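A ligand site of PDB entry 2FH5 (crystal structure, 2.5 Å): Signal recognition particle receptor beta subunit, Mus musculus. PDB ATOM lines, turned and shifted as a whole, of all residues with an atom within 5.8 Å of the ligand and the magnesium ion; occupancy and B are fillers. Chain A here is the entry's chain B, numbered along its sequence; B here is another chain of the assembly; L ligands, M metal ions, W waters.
NZ of Lys 20 of chain A lies within salt-bridge range of O3 of the ligand (2.6 Å).
The side-chain hydroxyl of Thr 35 lies within hydrogen-bond range of an oxygen (O9) of the ligand (2.7 Å).
The backbone NH (N) of Ser 18 lies within hydrogen-bond range of an oxygen (O5) of the ligand (3.2 Å).
The backbone NH (N) of Gly 19 is in hydrogen-bond range of an oxygen (O5) of the ligand (2.8 Å).
O2 of the ligand sits close to N of Ser 38.
An oxygen (O1) of the ligand lies close to the side-chain sulfur of Cys 16.
O14 of the ligand sits close to OD1 of Asn 123 (3.2 Å).
N of Lys 20 of chain A lies within hydrogen-bond range of O5 of the ligand.
N of Asp 17 lies within hydrogen-bond range of O4 of the ligand, 2.9 Å away.
The side-chain carboxylate (OD1) of Asp 126 sits at hydrogen-bond distance from a nitrogen (N3) of the ligand, 2.6 Å away.
An oxygen (O14) of the ligand sits close to the backbone NH (N) of Lys 124 (3.2 Å).
N of Ala 191 sits at hydrogen-bond distance from O14 of the ligand, 2.8 Å away.
The backbone NH (N) of Leu 22 sits at hydrogen-bond distance from an oxygen (O8) of the ligand.
The backbone NH (N) of Thr 21 of chain A sits at hydrogen-bond distance from an oxygen (O8) of the ligand, 3.2 Å away.
N of Gly 63 sits at hydrogen-bond distance from O3 of the ligand, 2.8 Å away.
OG1 of Thr 21 of chain A lies close to OD2 of Asp 60 (2.6 Å).
O of Leu 15 sits at hydrogen-bond distance from OG of Ser 18, at 2.8 Å.
The side-chain sulfur (SG) of Cys 16 lies within hydrogen-bond range of the backbone NH (N) of His 64, at 3.4 Å.
The side-chain amino group of Lys 20 of chain A sits at hydrogen-bond distance from the backbone carbonyl oxygen of Leu 15 (2.9 Å).
The side-chain amino group (NZ) of Lys 20 of chain A is in hydrogen-bond range of the backbone carbonyl oxygen (O) of Gly 14 (3.0 Å).
The backbone NH of Lys 124 is in hydrogen-bond range of the backbone carbonyl oxygen of Cys 189 (3.2 Å).
OD1 of Asp 126 sits at hydrogen-bond distance from OG of Ser 190, 2.5 Å away.
NZ of Lys 124 lies within hydrogen-bond range of O of Asp 17.
Merely in contact with the ligand: Thr 37, Ser 190, Lys 192, Ile 127, Tyr 32, Pro 62 and Leu 15.
Hydrophobic or aromatic side chains within 4 Å of the ligand: Leu 22, Tyr 32, Ile 127 and Ala 191.
The nearest printed residue that does not touch the ligand is Gln 36 (4.4 Å).
Asp 60 touches the magnesium ion (OD2 to MG, 3.9 Å).
Three residues have an atom within 4 Å of the magnesium ion: Thr 21 of chain A, Ser 38 and Asp 60.
The nearest printed residue that does not touch the magnesium ion is Gly 20 of chain B (4.2 Å).
The magnesium ion is bound by water W4 (2.1 Å), water W3 (2.1 Å), O2 of the ligand (2.1 Å), OG1 of Thr 21 of chain A (2.2 Å), O6 of the ligand (2.2 Å) and OG of Ser 38 (2.3 Å).
The magnesium ion has six donor atoms within binding distance.
Water W4 bridges O9 of the ligand (2.7 Å) and O of Gln 36 (3.0 Å).
Water W6 lies within hydrogen-bond range of O1 of the ligand, OG1 of Thr 37 and OD1 of Asp 17.
Water W1 lies within hydrogen-bond range of an oxygen (O13) of the ligand, the side-chain hydroxyl of Thr 35 and the backbone carbonyl oxygen of Arg 33.
Water W2 bridges O9 of the ligand (2.7 Å) and N of Thr 37 (3.5 Å).
Water W5 lies within hydrogen-bond range of the backbone carbonyl oxygen (O) of Ser 38 (2.8 Å), the backbone NH (N) of His 64 (3.0 Å), an oxygen (O1) of the ligand (3.2 Å) and the backbone NH (N) of Gly 63 (3.3 Å).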
ATOM      1  N   GLY A  14     -17.927 -33.056  29.589  1.00  0.00           N
ATOM      2  CA  GLY A  14     -17.441 -32.765  30.926  1.00  0.00           C
ATOM      3  C   GLY A  14     -18.518 -32.030  31.692  1.00  0.00           C
ATOM      4  O   GLY A  14     -19.517 -31.573  31.102  1.00  0.00           O
ATOM      5  N   LEU A  15     -18.326 -31.900  33.012  1.00  0.00           N
ATOM      6  CA  LEU A  15     -19.330 -31.229  33.838  1.00  0.00           C
ATOM      7  C   LEU A  15     -19.473 -29.789  33.402  1.00  0.00           C
ATOM      8  O   LEU A  15     -18.632 -29.281  32.661  1.00  0.00           O
ATOM      9  CB  LEU A  15     -18.945 -31.253  35.338  1.00  0.00           C
ATOM     10  CG  LEU A  15     -18.647 -32.627  35.958  1.00  0.00           C
ATOM     11  CD1 LEU A  15     -18.189 -32.416  37.377  1.00  0.00           C
ATOM     12  CD2 LEU A  15     -19.859 -33.536  35.880  1.00  0.00           C
ATOM     13  N   CYS A  16     -20.553 -29.167  33.840  1.00  0.00           N
ATOM     14  CA  CYS A  16     -20.783 -27.747  33.568  1.00  0.00           C
ATOM     15  C   CYS A  16     -19.597 -26.971  34.077  1.00  0.00           C
ATOM     16  O   CYS A  16     -19.020 -27.327  35.098  1.00  0.00           O
ATOM     17  CB  CYS A  16     -22.024 -27.257  34.314  1.00  0.00           C
ATOM     18  SG  CYS A  16     -23.543 -27.790  33.559  1.00  0.00           S
ATOM     19  N   ASP A  17     -19.214 -25.922  33.358  1.00  0.00           N
ATOM     20  CA  ASP A  17     -18.098 -25.101  33.784  1.00  0.00           C
ATOM     21  C   ASP A  17     -16.714 -25.724  33.732  1.00  0.00           C
ATOM     22  O   ASP A  17     -15.791 -25.151  34.325  1.00  0.00           O
ATOM     23  CB  ASP A  17     -18.324 -24.603  35.212  1.00  0.00           C
ATOM     24  CG  ASP A  17     -19.487 -23.666  35.309  1.00  0.00           C
ATOM     25  OD1 ASP A  17     -19.412 -22.584  34.673  1.00  0.00           O
ATOM     26  OD2 ASP A  17     -20.463 -24.010  36.018  1.00  0.00           O
ATOM     27  N   SER A  18     -16.552 -26.878  33.097  1.00  0.00           N
ATOM     28  CA  SER A  18     -15.206 -27.436  33.063  1.00  0.00           C
ATOM     29  C   SER A  18     -14.357 -26.630  32.046  1.00  0.00           C
ATOM     30  O   SER A  18     -13.132 -26.591  32.148  1.00  0.00           O
ATOM     31  CB  SER A  18     -15.237 -28.932  32.734  1.00  0.00           C
ATOM     32  OG  SER A  18     -16.023 -29.188  31.592  1.00  0.00           O
ATOM     33  N   GLY A  19     -15.027 -25.962  31.106  1.00  0.00           N
ATOM     34  CA  GLY A  19     -14.365 -25.126  30.112  1.00  0.00           C
ATOM     35  C   GLY A  19     -14.449 -25.629  28.677  1.00  0.00           C
ATOM     36  O   GLY A  19     -13.633 -25.247  27.844  1.00  0.00           O
ATOM     37  N   LYS A  20     -15.440 -26.463  28.385  1.00  0.00           N
ATOM     38  CA  LYS A  20     -15.560 -27.036  27.045  1.00  0.00           C
ATOM     39  C   LYS A  20     -15.724 -25.995  25.965  1.00  0.00           C
ATOM     40  O   LYS A  20     -15.025 -26.038  24.959  1.00  0.00           O
ATOM     41  CB  LYS A  20     -16.728 -28.055  26.962  1.00  0.00           C
ATOM     42  CG  LYS A  20     -16.584 -29.276  27.910  1.00  0.00           C
ATOM     43  CD  LYS A  20     -17.858 -30.157  27.918  1.00  0.00           C
ATOM     44  CE  LYS A  20     -19.106 -29.421  28.412  1.00  0.00           C
ATOM     45  NZ  LYS A  20     -18.977 -28.909  29.801  1.00  0.00           N
ATOM     46  N   THR A  21     -16.628 -25.042  26.180  1.00  0.00           N
ATOM     47  CA  THR A  21     -16.849 -24.043  25.162  1.00  0.00           C
ATOM     48  C   THR A  21     -15.678 -23.107  24.984  1.00  0.00           C
ATOM     49  O   THR A  21     -15.379 -22.739  23.855  1.00  0.00           O
ATOM     50  CB  THR A  21     -18.123 -23.250  25.454  1.00  0.00           C
ATOM     51  OG1 THR A  21     -19.201 -24.174  25.508  1.00  0.00           O
ATOM     52  CG2 THR A  21     -18.427 -22.259  24.324  1.00  0.00           C
ATOM     53  N   LEU A  22     -15.013 -22.708  26.077  1.00  0.00           N
ATOM     54  CA  LEU A  22     -13.886 -21.809  25.919  1.00  0.00           C
ATOM     55  C   LEU A  22     -12.738 -22.520  25.187  1.00  0.00           C
ATOM     56  O   LEU A  22     -12.116 -21.904  24.334  1.00  0.00           O
ATOM     57  CB  LEU A  22     -13.400 -21.262  27.261  1.00  0.00           C
ATOM     58  CG  LEU A  22     -12.391 -20.125  27.040  1.00  0.00           C
ATOM     59  CD1 LEU A  22     -12.960 -19.124  26.085  1.00  0.00           C
ATOM     60  CD2 LEU A  22     -12.021 -19.430  28.355  1.00  0.00           C
ATOM     61  N   LEU A  23     -12.472 -23.796  25.481  1.00  0.00           N
ATOM     62  CA  LEU A  23     -11.414 -24.516  24.771  1.00  0.00           C
ATOM     63  C   LEU A  23     -11.764 -24.574  23.303  1.00  0.00           C
ATOM     64  O   LEU A  23     -10.923 -24.337  22.451  1.00  0.00           O
ATOM     65  CB  LEU A  23     -11.278 -25.955  25.280  1.00  0.00           C
ATOM     66  CG  LEU A  23     -10.544 -26.158  26.593  1.00  0.00           C
ATOM     67  CD1 LEU A  23     -10.545 -27.631  26.942  1.00  0.00           C
ATOM     68  CD2 LEU A  23      -9.116 -25.654  26.442  1.00  0.00           C
ATOM     69  N   TYR A  32     -10.209 -15.301  23.207  1.00  0.00           N
ATOM     70  CA  TYR A  32     -11.052 -15.442  24.375  1.00  0.00           C
ATOM     71  C   TYR A  32     -12.414 -14.886  23.970  1.00  0.00           C
ATOM     72  O   TYR A  32     -12.494 -14.044  23.077  1.00  0.00           O
ATOM     73  CB  TYR A  32     -10.533 -14.629  25.555  1.00  0.00           C
ATOM     74  CG  TYR A  32     -11.540 -14.530  26.689  1.00  0.00           C
ATOM     75  CD1 TYR A  32     -11.664 -15.548  27.631  1.00  0.00           C
ATOM     76  CD2 TYR A  32     -12.421 -13.430  26.794  1.00  0.00           C
ATOM     77  CE1 TYR A  32     -12.618 -15.489  28.636  1.00  0.00           C
ATOM     78  CE2 TYR A  32     -13.384 -13.370  27.800  1.00  0.00           C
ATOM     79  CZ  TYR A  32     -13.475 -14.410  28.713  1.00  0.00           C
ATOM     80  OH  TYR A  32     -14.452 -14.405  29.692  1.00  0.00           O
ATOM     81  N   ARG A  33     -13.474 -15.369  24.615  1.00  0.00           N
ATOM     82  CA  ARG A  33     -14.848 -14.900  24.391  1.00  0.00           C
ATOM     83  C   ARG A  33     -15.637 -15.237  25.628  1.00  0.00           C
ATOM     84  O   ARG A  33     -15.434 -16.281  26.230  1.00  0.00           O
ATOM     85  CB  ARG A  33     -15.534 -15.612  23.223  1.00  0.00           C
ATOM     86  CG  ARG A  33     -14.964 -15.351  21.861  1.00  0.00           C
ATOM     87  CD  ARG A  33     -15.533 -14.097  21.208  1.00  0.00           C
ATOM     88  NE  ARG A  33     -15.353 -14.132  19.757  1.00  0.00           N
ATOM     89  CZ  ARG A  33     -14.169 -14.210  19.146  1.00  0.00           C
ATOM     90  NH1 ARG A  33     -13.053 -14.257  19.865  1.00  0.00           N
ATOM     91  NH2 ARG A  33     -14.104 -14.274  17.820  1.00  0.00           N
ATOM     92  N   THR A  35     -18.780 -16.538  27.687  1.00  0.00           N
ATOM     93  CA  THR A  35     -19.683 -17.641  27.436  1.00  0.00           C
ATOM     94  C   THR A  35     -20.714 -17.762  28.563  1.00  0.00           C
ATOM     95  O   THR A  35     -20.543 -17.220  29.643  1.00  0.00           O
ATOM     96  CB  THR A  35     -18.887 -18.987  27.360  1.00  0.00           C
ATOM     97  OG1 THR A  35     -18.114 -19.148  28.562  1.00  0.00           O
ATOM     98  CG2 THR A  35     -17.944 -18.997  26.191  1.00  0.00           C
ATOM     99  N   GLN A  36     -21.777 -18.495  28.300  1.00  0.00           N
ATOM    100  CA  GLN A  36     -22.803 -18.773  29.306  1.00  0.00           C
ATOM    101  C   GLN A  36     -23.009 -20.275  29.218  1.00  0.00           C
ATOM    102  O   GLN A  36     -22.572 -20.934  28.252  1.00  0.00           O
ATOM    103  CB  GLN A  36     -24.103 -18.059  28.941  1.00  0.00           C
ATOM    104  CG  GLN A  36     -24.006 -16.520  28.847  1.00  0.00           C
ATOM    105  CD  GLN A  36     -23.743 -15.808  30.180  1.00  0.00           C
ATOM    106  OE1 GLN A  36     -23.505 -14.622  30.206  1.00  0.00           O
ATOM    107  NE2 GLN A  36     -23.776 -16.549  31.283  1.00  0.00           N
ATOM    108  N   THR A  37     -23.681 -20.841  30.211  1.00  0.00           N
ATOM    109  CA  THR A  37     -23.988 -22.260  30.173  1.00  0.00           C
ATOM    110  C   THR A  37     -24.630 -22.625  28.836  1.00  0.00           C
ATOM    111  O   THR A  37     -25.596 -21.991  28.396  1.00  0.00           O
ATOM    112  CB  THR A  37     -24.938 -22.605  31.320  1.00  0.00           C
ATOM    113  OG1 THR A  37     -24.299 -22.275  32.558  1.00  0.00           O
ATOM    114  CG2 THR A  37     -25.284 -24.088  31.348  1.00  0.00           C
ATOM    115  N   SER A  38     -24.091 -23.662  28.197  1.00  0.00           N
ATOM    116  CA  SER A  38     -24.558 -24.148  26.905  1.00  0.00           C
ATOM    117  C   SER A  38     -25.826 -24.962  27.007  1.00  0.00           C
ATOM    118  O   SER A  38     -25.935 -25.809  27.886  1.00  0.00           O
ATOM    119  CB  SER A  38     -23.473 -25.014  26.247  1.00  0.00           C
ATOM    120  OG  SER A  38     -22.343 -24.243  25.921  1.00  0.00           O
ATOM    121  N   ILE A  39     -26.768 -24.752  26.086  1.00  0.00           N
ATOM    122  CA  ILE A  39     -27.991 -25.533  26.125  1.00  0.00           C
ATOM    123  C   ILE A  39     -28.174 -26.487  24.931  1.00  0.00           C
ATOM    124  O   ILE A  39     -29.091 -27.307  24.929  1.00  0.00           O
ATOM    125  CB  ILE A  39     -29.259 -24.641  26.363  1.00  0.00           C
ATOM    126  CG1 ILE A  39     -29.602 -23.842  25.121  1.00  0.00           C
ATOM    127  CG2 ILE A  39     -28.990 -23.651  27.489  1.00  0.00           C
ATOM    128  CD1 ILE A  39     -30.777 -22.910  25.393  1.00  0.00           C
ATOM    129  N   ASP A  60     -18.833 -29.458  20.568  1.00  0.00           N
ATOM    130  CA  ASP A  60     -18.882 -29.062  21.983  1.00  0.00           C
ATOM    131  C   ASP A  60     -20.208 -29.527  22.558  1.00  0.00           C
ATOM    132  O   ASP A  60     -21.238 -29.047  22.120  1.00  0.00           O
ATOM    133  CB  ASP A  60     -18.738 -27.523  22.036  1.00  0.00           C
ATOM    134  CG  ASP A  60     -19.068 -26.917  23.418  1.00  0.00           C
ATOM    135  OD1 ASP A  60     -18.783 -27.532  24.465  1.00  0.00           O
ATOM    136  OD2 ASP A  60     -19.616 -25.774  23.450  1.00  0.00           O
ATOM    137  N   LEU A  61     -20.205 -30.430  23.533  1.00  0.00           N
ATOM    138  CA  LEU A  61     -21.471 -30.917  24.116  1.00  0.00           C
ATOM    139  C   LEU A  61     -21.797 -30.341  25.491  1.00  0.00           C
ATOM    140  O   LEU A  61     -20.956 -30.280  26.363  1.00  0.00           O
ATOM    141  CB  LEU A  61     -21.476 -32.464  24.215  1.00  0.00           C
ATOM    142  CG  LEU A  61     -21.298 -33.269  22.902  1.00  0.00           C
ATOM    143  CD1 LEU A  61     -21.421 -34.767  23.161  1.00  0.00           C
ATOM    144  CD2 LEU A  61     -22.356 -32.849  21.893  1.00  0.00           C
ATOM    145  N   PRO A  62     -23.048 -29.888  25.688  1.00  0.00           N
ATOM    146  CA  PRO A  62     -23.462 -29.302  26.965  1.00  0.00           C
ATOM    147  C   PRO A  62     -23.182 -30.245  28.149  1.00  0.00           C
ATOM    148  O   PRO A  62     -23.423 -31.442  28.060  1.00  0.00           O
ATOM    149  CB  PRO A  62     -24.959 -29.084  26.785  1.00  0.00           C
ATOM    150  CG  PRO A  62     -25.154 -29.008  25.328  1.00  0.00           C
ATOM    151  CD  PRO A  62     -24.196 -30.045  24.792  1.00  0.00           C
ATOM    152  N   GLY A  63     -22.700 -29.712  29.253  1.00  0.00           N
ATOM    153  CA  GLY A  63     -22.432 -30.554  30.395  1.00  0.00           C
ATOM    154  C   GLY A  63     -23.594 -30.729  31.358  1.00  0.00           C
ATOM    155  O   GLY A  63     -23.539 -31.560  32.277  1.00  0.00           O
ATOM    156  N   HIS A  64     -24.660 -29.961  31.163  1.00  0.00           N
ATOM    157  CA  HIS A  64     -25.795 -30.089  32.058  1.00  0.00           C
ATOM    158  C   HIS A  64     -26.306 -31.549  32.125  1.00  0.00           C
ATOM    159  O   HIS A  64     -26.414 -32.226  31.114  1.00  0.00           O
ATOM    160  CB  HIS A  64     -26.921 -29.134  31.659  1.00  0.00           C
ATOM    161  CG  HIS A  64     -27.856 -28.831  32.788  1.00  0.00           C
ATOM    162  ND1 HIS A  64     -29.074 -29.434  32.931  1.00  0.00           N
ATOM    163  CD2 HIS A  64     -27.666 -28.071  33.895  1.00  0.00           C
ATOM    164  CE1 HIS A  64     -29.606 -29.086  34.091  1.00  0.00           C
ATOM    165  NE2 HIS A  64     -28.775 -28.262  34.703  1.00  0.00           N
ATOM    166  N   ASN A 123      -8.021 -29.055  32.584  1.00  0.00           N
ATOM    167  CA  ASN A 123      -8.095 -27.636  32.267  1.00  0.00           C
ATOM    168  C   ASN A 123      -8.045 -26.678  33.461  1.00  0.00           C
ATOM    169  O   ASN A 123      -8.097 -27.098  34.636  1.00  0.00           O
ATOM    170  CB  ASN A 123      -9.354 -27.441  31.422  1.00  0.00           C
ATOM    171  CG  ASN A 123      -9.478 -26.055  30.850  1.00  0.00           C
ATOM    172  OD1 ASN A 123      -8.489 -25.557  30.259  1.00  0.00           O
ATOM    173  ND2 ASN A 123     -10.593 -25.490  30.964  1.00  0.00           N
ATOM    174  N   LYS A 124      -7.950 -25.384  33.159  1.00  0.00           N
ATOM    175  CA  LYS A 124      -7.865 -24.323  34.171  1.00  0.00           C
ATOM    176  C   LYS A 124      -6.565 -24.368  34.997  1.00  0.00           C
ATOM    177  O   LYS A 124      -6.552 -23.967  36.177  1.00  0.00           O
ATOM    178  CB  LYS A 124      -9.076 -24.381  35.101  1.00  0.00           C
ATOM    179  CG  LYS A 124     -10.425 -24.228  34.364  1.00  0.00           C
ATOM    180  CD  LYS A 124     -11.529 -23.550  35.195  1.00  0.00           C
ATOM    181  CE  LYS A 124     -12.841 -23.668  34.444  1.00  0.00           C
ATOM    182  NZ  LYS A 124     -14.033 -23.487  35.332  1.00  0.00           N
ATOM    183  N   GLN A 125      -5.475 -24.850  34.378  1.00  0.00           N
ATOM    184  CA  GLN A 125      -4.163 -24.942  35.029  1.00  0.00           C
ATOM    185  C   GLN A 125      -3.613 -23.561  35.424  1.00  0.00           C
ATOM    186  O   GLN A 125      -2.824 -23.460  36.373  1.00  0.00           O
ATOM    187  CB  GLN A 125      -3.160 -25.650  34.114  1.00  0.00           C
ATOM    188  CG  GLN A 125      -3.365 -27.154  33.974  1.00  0.00           C
ATOM    189  CD  GLN A 125      -3.301 -27.877  35.312  1.00  0.00           C
ATOM    190  OE1 GLN A 125      -2.391 -27.670  36.098  1.00  0.00           O
ATOM    191  NE2 GLN A 125      -4.283 -28.746  35.567  1.00  0.00           N
ATOM    192  N   ASP A 126      -4.039 -22.510  34.713  1.00  0.00           N
ATOM    193  CA  ASP A 126      -3.615 -21.151  35.000  1.00  0.00           C
ATOM    194  C   ASP A 126      -4.024 -20.688  36.408  1.00  0.00           C
ATOM    195  O   ASP A 126      -3.493 -19.704  36.930  1.00  0.00           O
ATOM    196  CB  ASP A 126      -4.221 -20.184  33.982  1.00  0.00           C
ATOM    197  CG  ASP A 126      -5.753 -20.217  33.998  1.00  0.00           C
ATOM    198  OD1 ASP A 126      -6.340 -21.196  33.507  1.00  0.00           O
ATOM    199  OD2 ASP A 126      -6.357 -19.263  34.518  1.00  0.00           O
ATOM    200  N   ILE A 127      -4.975 -21.373  37.031  1.00  0.00           N
ATOM    201  CA  ILE A 127      -5.409 -21.011  38.384  1.00  0.00           C
ATOM    202  C   ILE A 127      -4.445 -21.676  39.363  1.00  0.00           C
ATOM    203  O   ILE A 127      -4.119 -22.853  39.213  1.00  0.00           O
ATOM    204  CB  ILE A 127      -6.871 -21.452  38.634  1.00  0.00           C
ATOM    205  CG1 ILE A 127      -7.809 -20.650  37.738  1.00  0.00           C
ATOM    206  CG2 ILE A 127      -7.240 -21.252  40.091  1.00  0.00           C
ATOM    207  CD1 ILE A 127      -9.235 -21.137  37.769  1.00  0.00           C
ATOM    208  N   CYS A 189      -3.878 -28.167  30.496  1.00  0.00           N
ATOM    209  CA  CYS A 189      -4.128 -27.039  29.609  1.00  0.00           C
ATOM    210  C   CYS A 189      -4.833 -25.900  30.321  1.00  0.00           C
ATOM    211  O   CYS A 189      -5.254 -26.024  31.481  1.00  0.00           O
ATOM    212  CB  CYS A 189      -4.954 -27.459  28.381  1.00  0.00           C
ATOM    213  SG  CYS A 189      -6.602 -28.099  28.736  1.00  0.00           S
ATOM    214  N   SER A 190      -4.929 -24.777  29.615  1.00  0.00           N
ATOM    215  CA  SER A 190      -5.581 -23.584  30.114  1.00  0.00           C
ATOM    216  C   SER A 190      -6.214 -22.865  28.932  1.00  0.00           C
ATOM    217  O   SER A 190      -5.567 -22.640  27.921  1.00  0.00           O
ATOM    218  CB  SER A 190      -4.574 -22.679  30.787  1.00  0.00           C
ATOM    219  OG  SER A 190      -5.213 -21.493  31.251  1.00  0.00           O
ATOM    220  N   ALA A 191      -7.493 -22.519  29.062  1.00  0.00           N
ATOM    221  CA  ALA A 191      -8.191 -21.827  27.997  1.00  0.00           C
ATOM    222  C   ALA A 191      -7.977 -20.311  28.117  1.00  0.00           C
ATOM    223  O   ALA A 191      -8.290 -19.558  27.202  1.00  0.00           O
ATOM    224  CB  ALA A 191      -9.672 -22.162  28.043  1.00  0.00           C
ATOM    225  N   LYS A 192      -7.463 -19.882  29.259  1.00  0.00           N
ATOM    226  CA  LYS A 192      -7.204 -18.464  29.489  1.00  0.00           C
ATOM    227  C   LYS A 192      -5.703 -18.213  29.630  1.00  0.00           C
ATOM    228  O   LYS A 192      -5.178 -18.152  30.744  1.00  0.00           O
ATOM    229  CB  LYS A 192      -7.914 -17.986  30.750  1.00  0.00           C
ATOM    230  CG  LYS A 192      -9.374 -17.591  30.576  1.00  0.00           C
ATOM    231  CD  LYS A 192      -9.899 -16.910  31.836  1.00  0.00           C
ATOM    232  CE  LYS A 192     -11.339 -16.505  31.703  1.00  0.00           C
ATOM    233  NZ  LYS A 192     -11.807 -15.819  32.934  1.00  0.00           N
ATOM    234  N   GLY B  20     -25.412 -22.315  22.044  1.00  0.00           N
ATOM    235  CA  GLY B  20     -24.149 -23.031  22.199  1.00  0.00           C
ATOM    236  C   GLY B  20     -23.362 -22.460  23.367  1.00  0.00           C
ATOM    237  O   GLY B  20     -22.431 -23.093  23.842  1.00  0.00           O
ATOM    238  N   GLY B  21     -23.763 -21.268  23.838  1.00  0.00           N
ATOM    239  CA  GLY B  21     -23.105 -20.626  24.967  1.00  0.00           C
ATOM    240  C   GLY B  21     -22.220 -19.429  24.632  1.00  0.00           C
ATOM    241  O   GLY B  21     -21.595 -18.846  25.508  1.00  0.00           O
HETATM  242  P1  LIG L   1     -21.290 -25.912  30.084  1.00  0.00           P
HETATM  243  O1  LIG L   1     -22.153 -25.600  31.204  1.00  0.00           O
HETATM  244  O2  LIG L   1     -21.699 -25.239  28.808  1.00  0.00           O
HETATM  245  O3  LIG L   1     -21.159 -27.438  29.889  1.00  0.00           O
HETATM  246  O4  LIG L   1     -19.785 -25.221  30.561  1.00  0.00           O
HETATM  247  P2  LIG L   1     -18.478 -25.221  29.761  1.00  0.00           P
HETATM  248  O5  LIG L   1     -17.656 -26.421  30.109  1.00  0.00           O
HETATM  249  O6  LIG L   1     -18.672 -25.097  28.261  1.00  0.00           O
HETATM  250  O7  LIG L   1     -17.776 -23.936  30.404  1.00  0.00           O
HETATM  251  P3  LIG L   1     -17.236 -22.631  29.708  1.00  0.00           P
HETATM  252  O8  LIG L   1     -16.398 -22.919  28.597  1.00  0.00           O
HETATM  253  O9  LIG L   1     -18.380 -21.721  29.356  1.00  0.00           O
HETATM  254  O10 LIG L   1     -16.348 -22.115  30.913  1.00  0.00           O
HETATM  255  C1  LIG L   1     -16.985 -21.777  32.127  1.00  0.00           C
HETATM  256  C2  LIG L   1     -16.248 -20.591  32.768  1.00  0.00           C
HETATM  257  O11 LIG L   1     -14.876 -20.946  33.054  1.00  0.00           O
HETATM  258  C3  LIG L   1     -16.163 -19.347  31.872  1.00  0.00           C
HETATM  259  O12 LIG L   1     -16.330 -18.133  32.662  1.00  0.00           O
HETATM  260  C4  LIG L   1     -14.785 -19.453  31.278  1.00  0.00           C
HETATM  261  O13 LIG L   1     -14.243 -18.243  30.729  1.00  0.00           O
HETATM  262  C5  LIG L   1     -13.951 -20.068  32.408  1.00  0.00           C
HETATM  263  N1  LIG L   1     -12.840 -20.890  31.970  1.00  0.00           N
HETATM  264  C6  LIG L   1     -12.888 -21.893  31.004  1.00  0.00           C
HETATM  265  N2  LIG L   1     -11.686 -22.447  30.848  1.00  0.00           N
HETATM  266  C7  LIG L   1     -10.827 -21.789  31.765  1.00  0.00           C
HETATM  267  C8  LIG L   1      -9.458 -21.931  32.080  1.00  0.00           C
HETATM  268  O14 LIG L   1      -8.629 -22.701  31.632  1.00  0.00           O
HETATM  269  N3  LIG L   1      -8.923 -21.062  33.073  1.00  0.00           N
HETATM  270  C9  LIG L   1      -9.689 -20.108  33.719  1.00  0.00           C
HETATM  271  N4  LIG L   1      -9.094 -19.311  34.649  1.00  0.00           N
HETATM  272  N5  LIG L   1     -11.008 -19.986  33.414  1.00  0.00           N
HETATM  273  C10 LIG L   1     -11.554 -20.816  32.440  1.00  0.00           C
HETATM  274 MG    MG M   1     -20.487 -24.778  27.130  1.00  0.00          MG
HETATM  275  O   HOH W   1     -15.698 -17.953  28.636  1.00  0.00           O
HETATM  276  O   HOH W   2     -20.403 -21.450  31.102  1.00  0.00           O
HETATM  277  O   HOH W   3     -20.518 -26.768  26.475  1.00  0.00           O
HETATM  278  O   HOH W   4     -20.325 -22.799  27.774  1.00  0.00           O
HETATM  279  O   HOH W   5     -24.665 -27.165  29.977  1.00  0.00           O
HETATM  280  O   HOH W   6     -21.757 -23.435  32.494  1.00  0.00           O
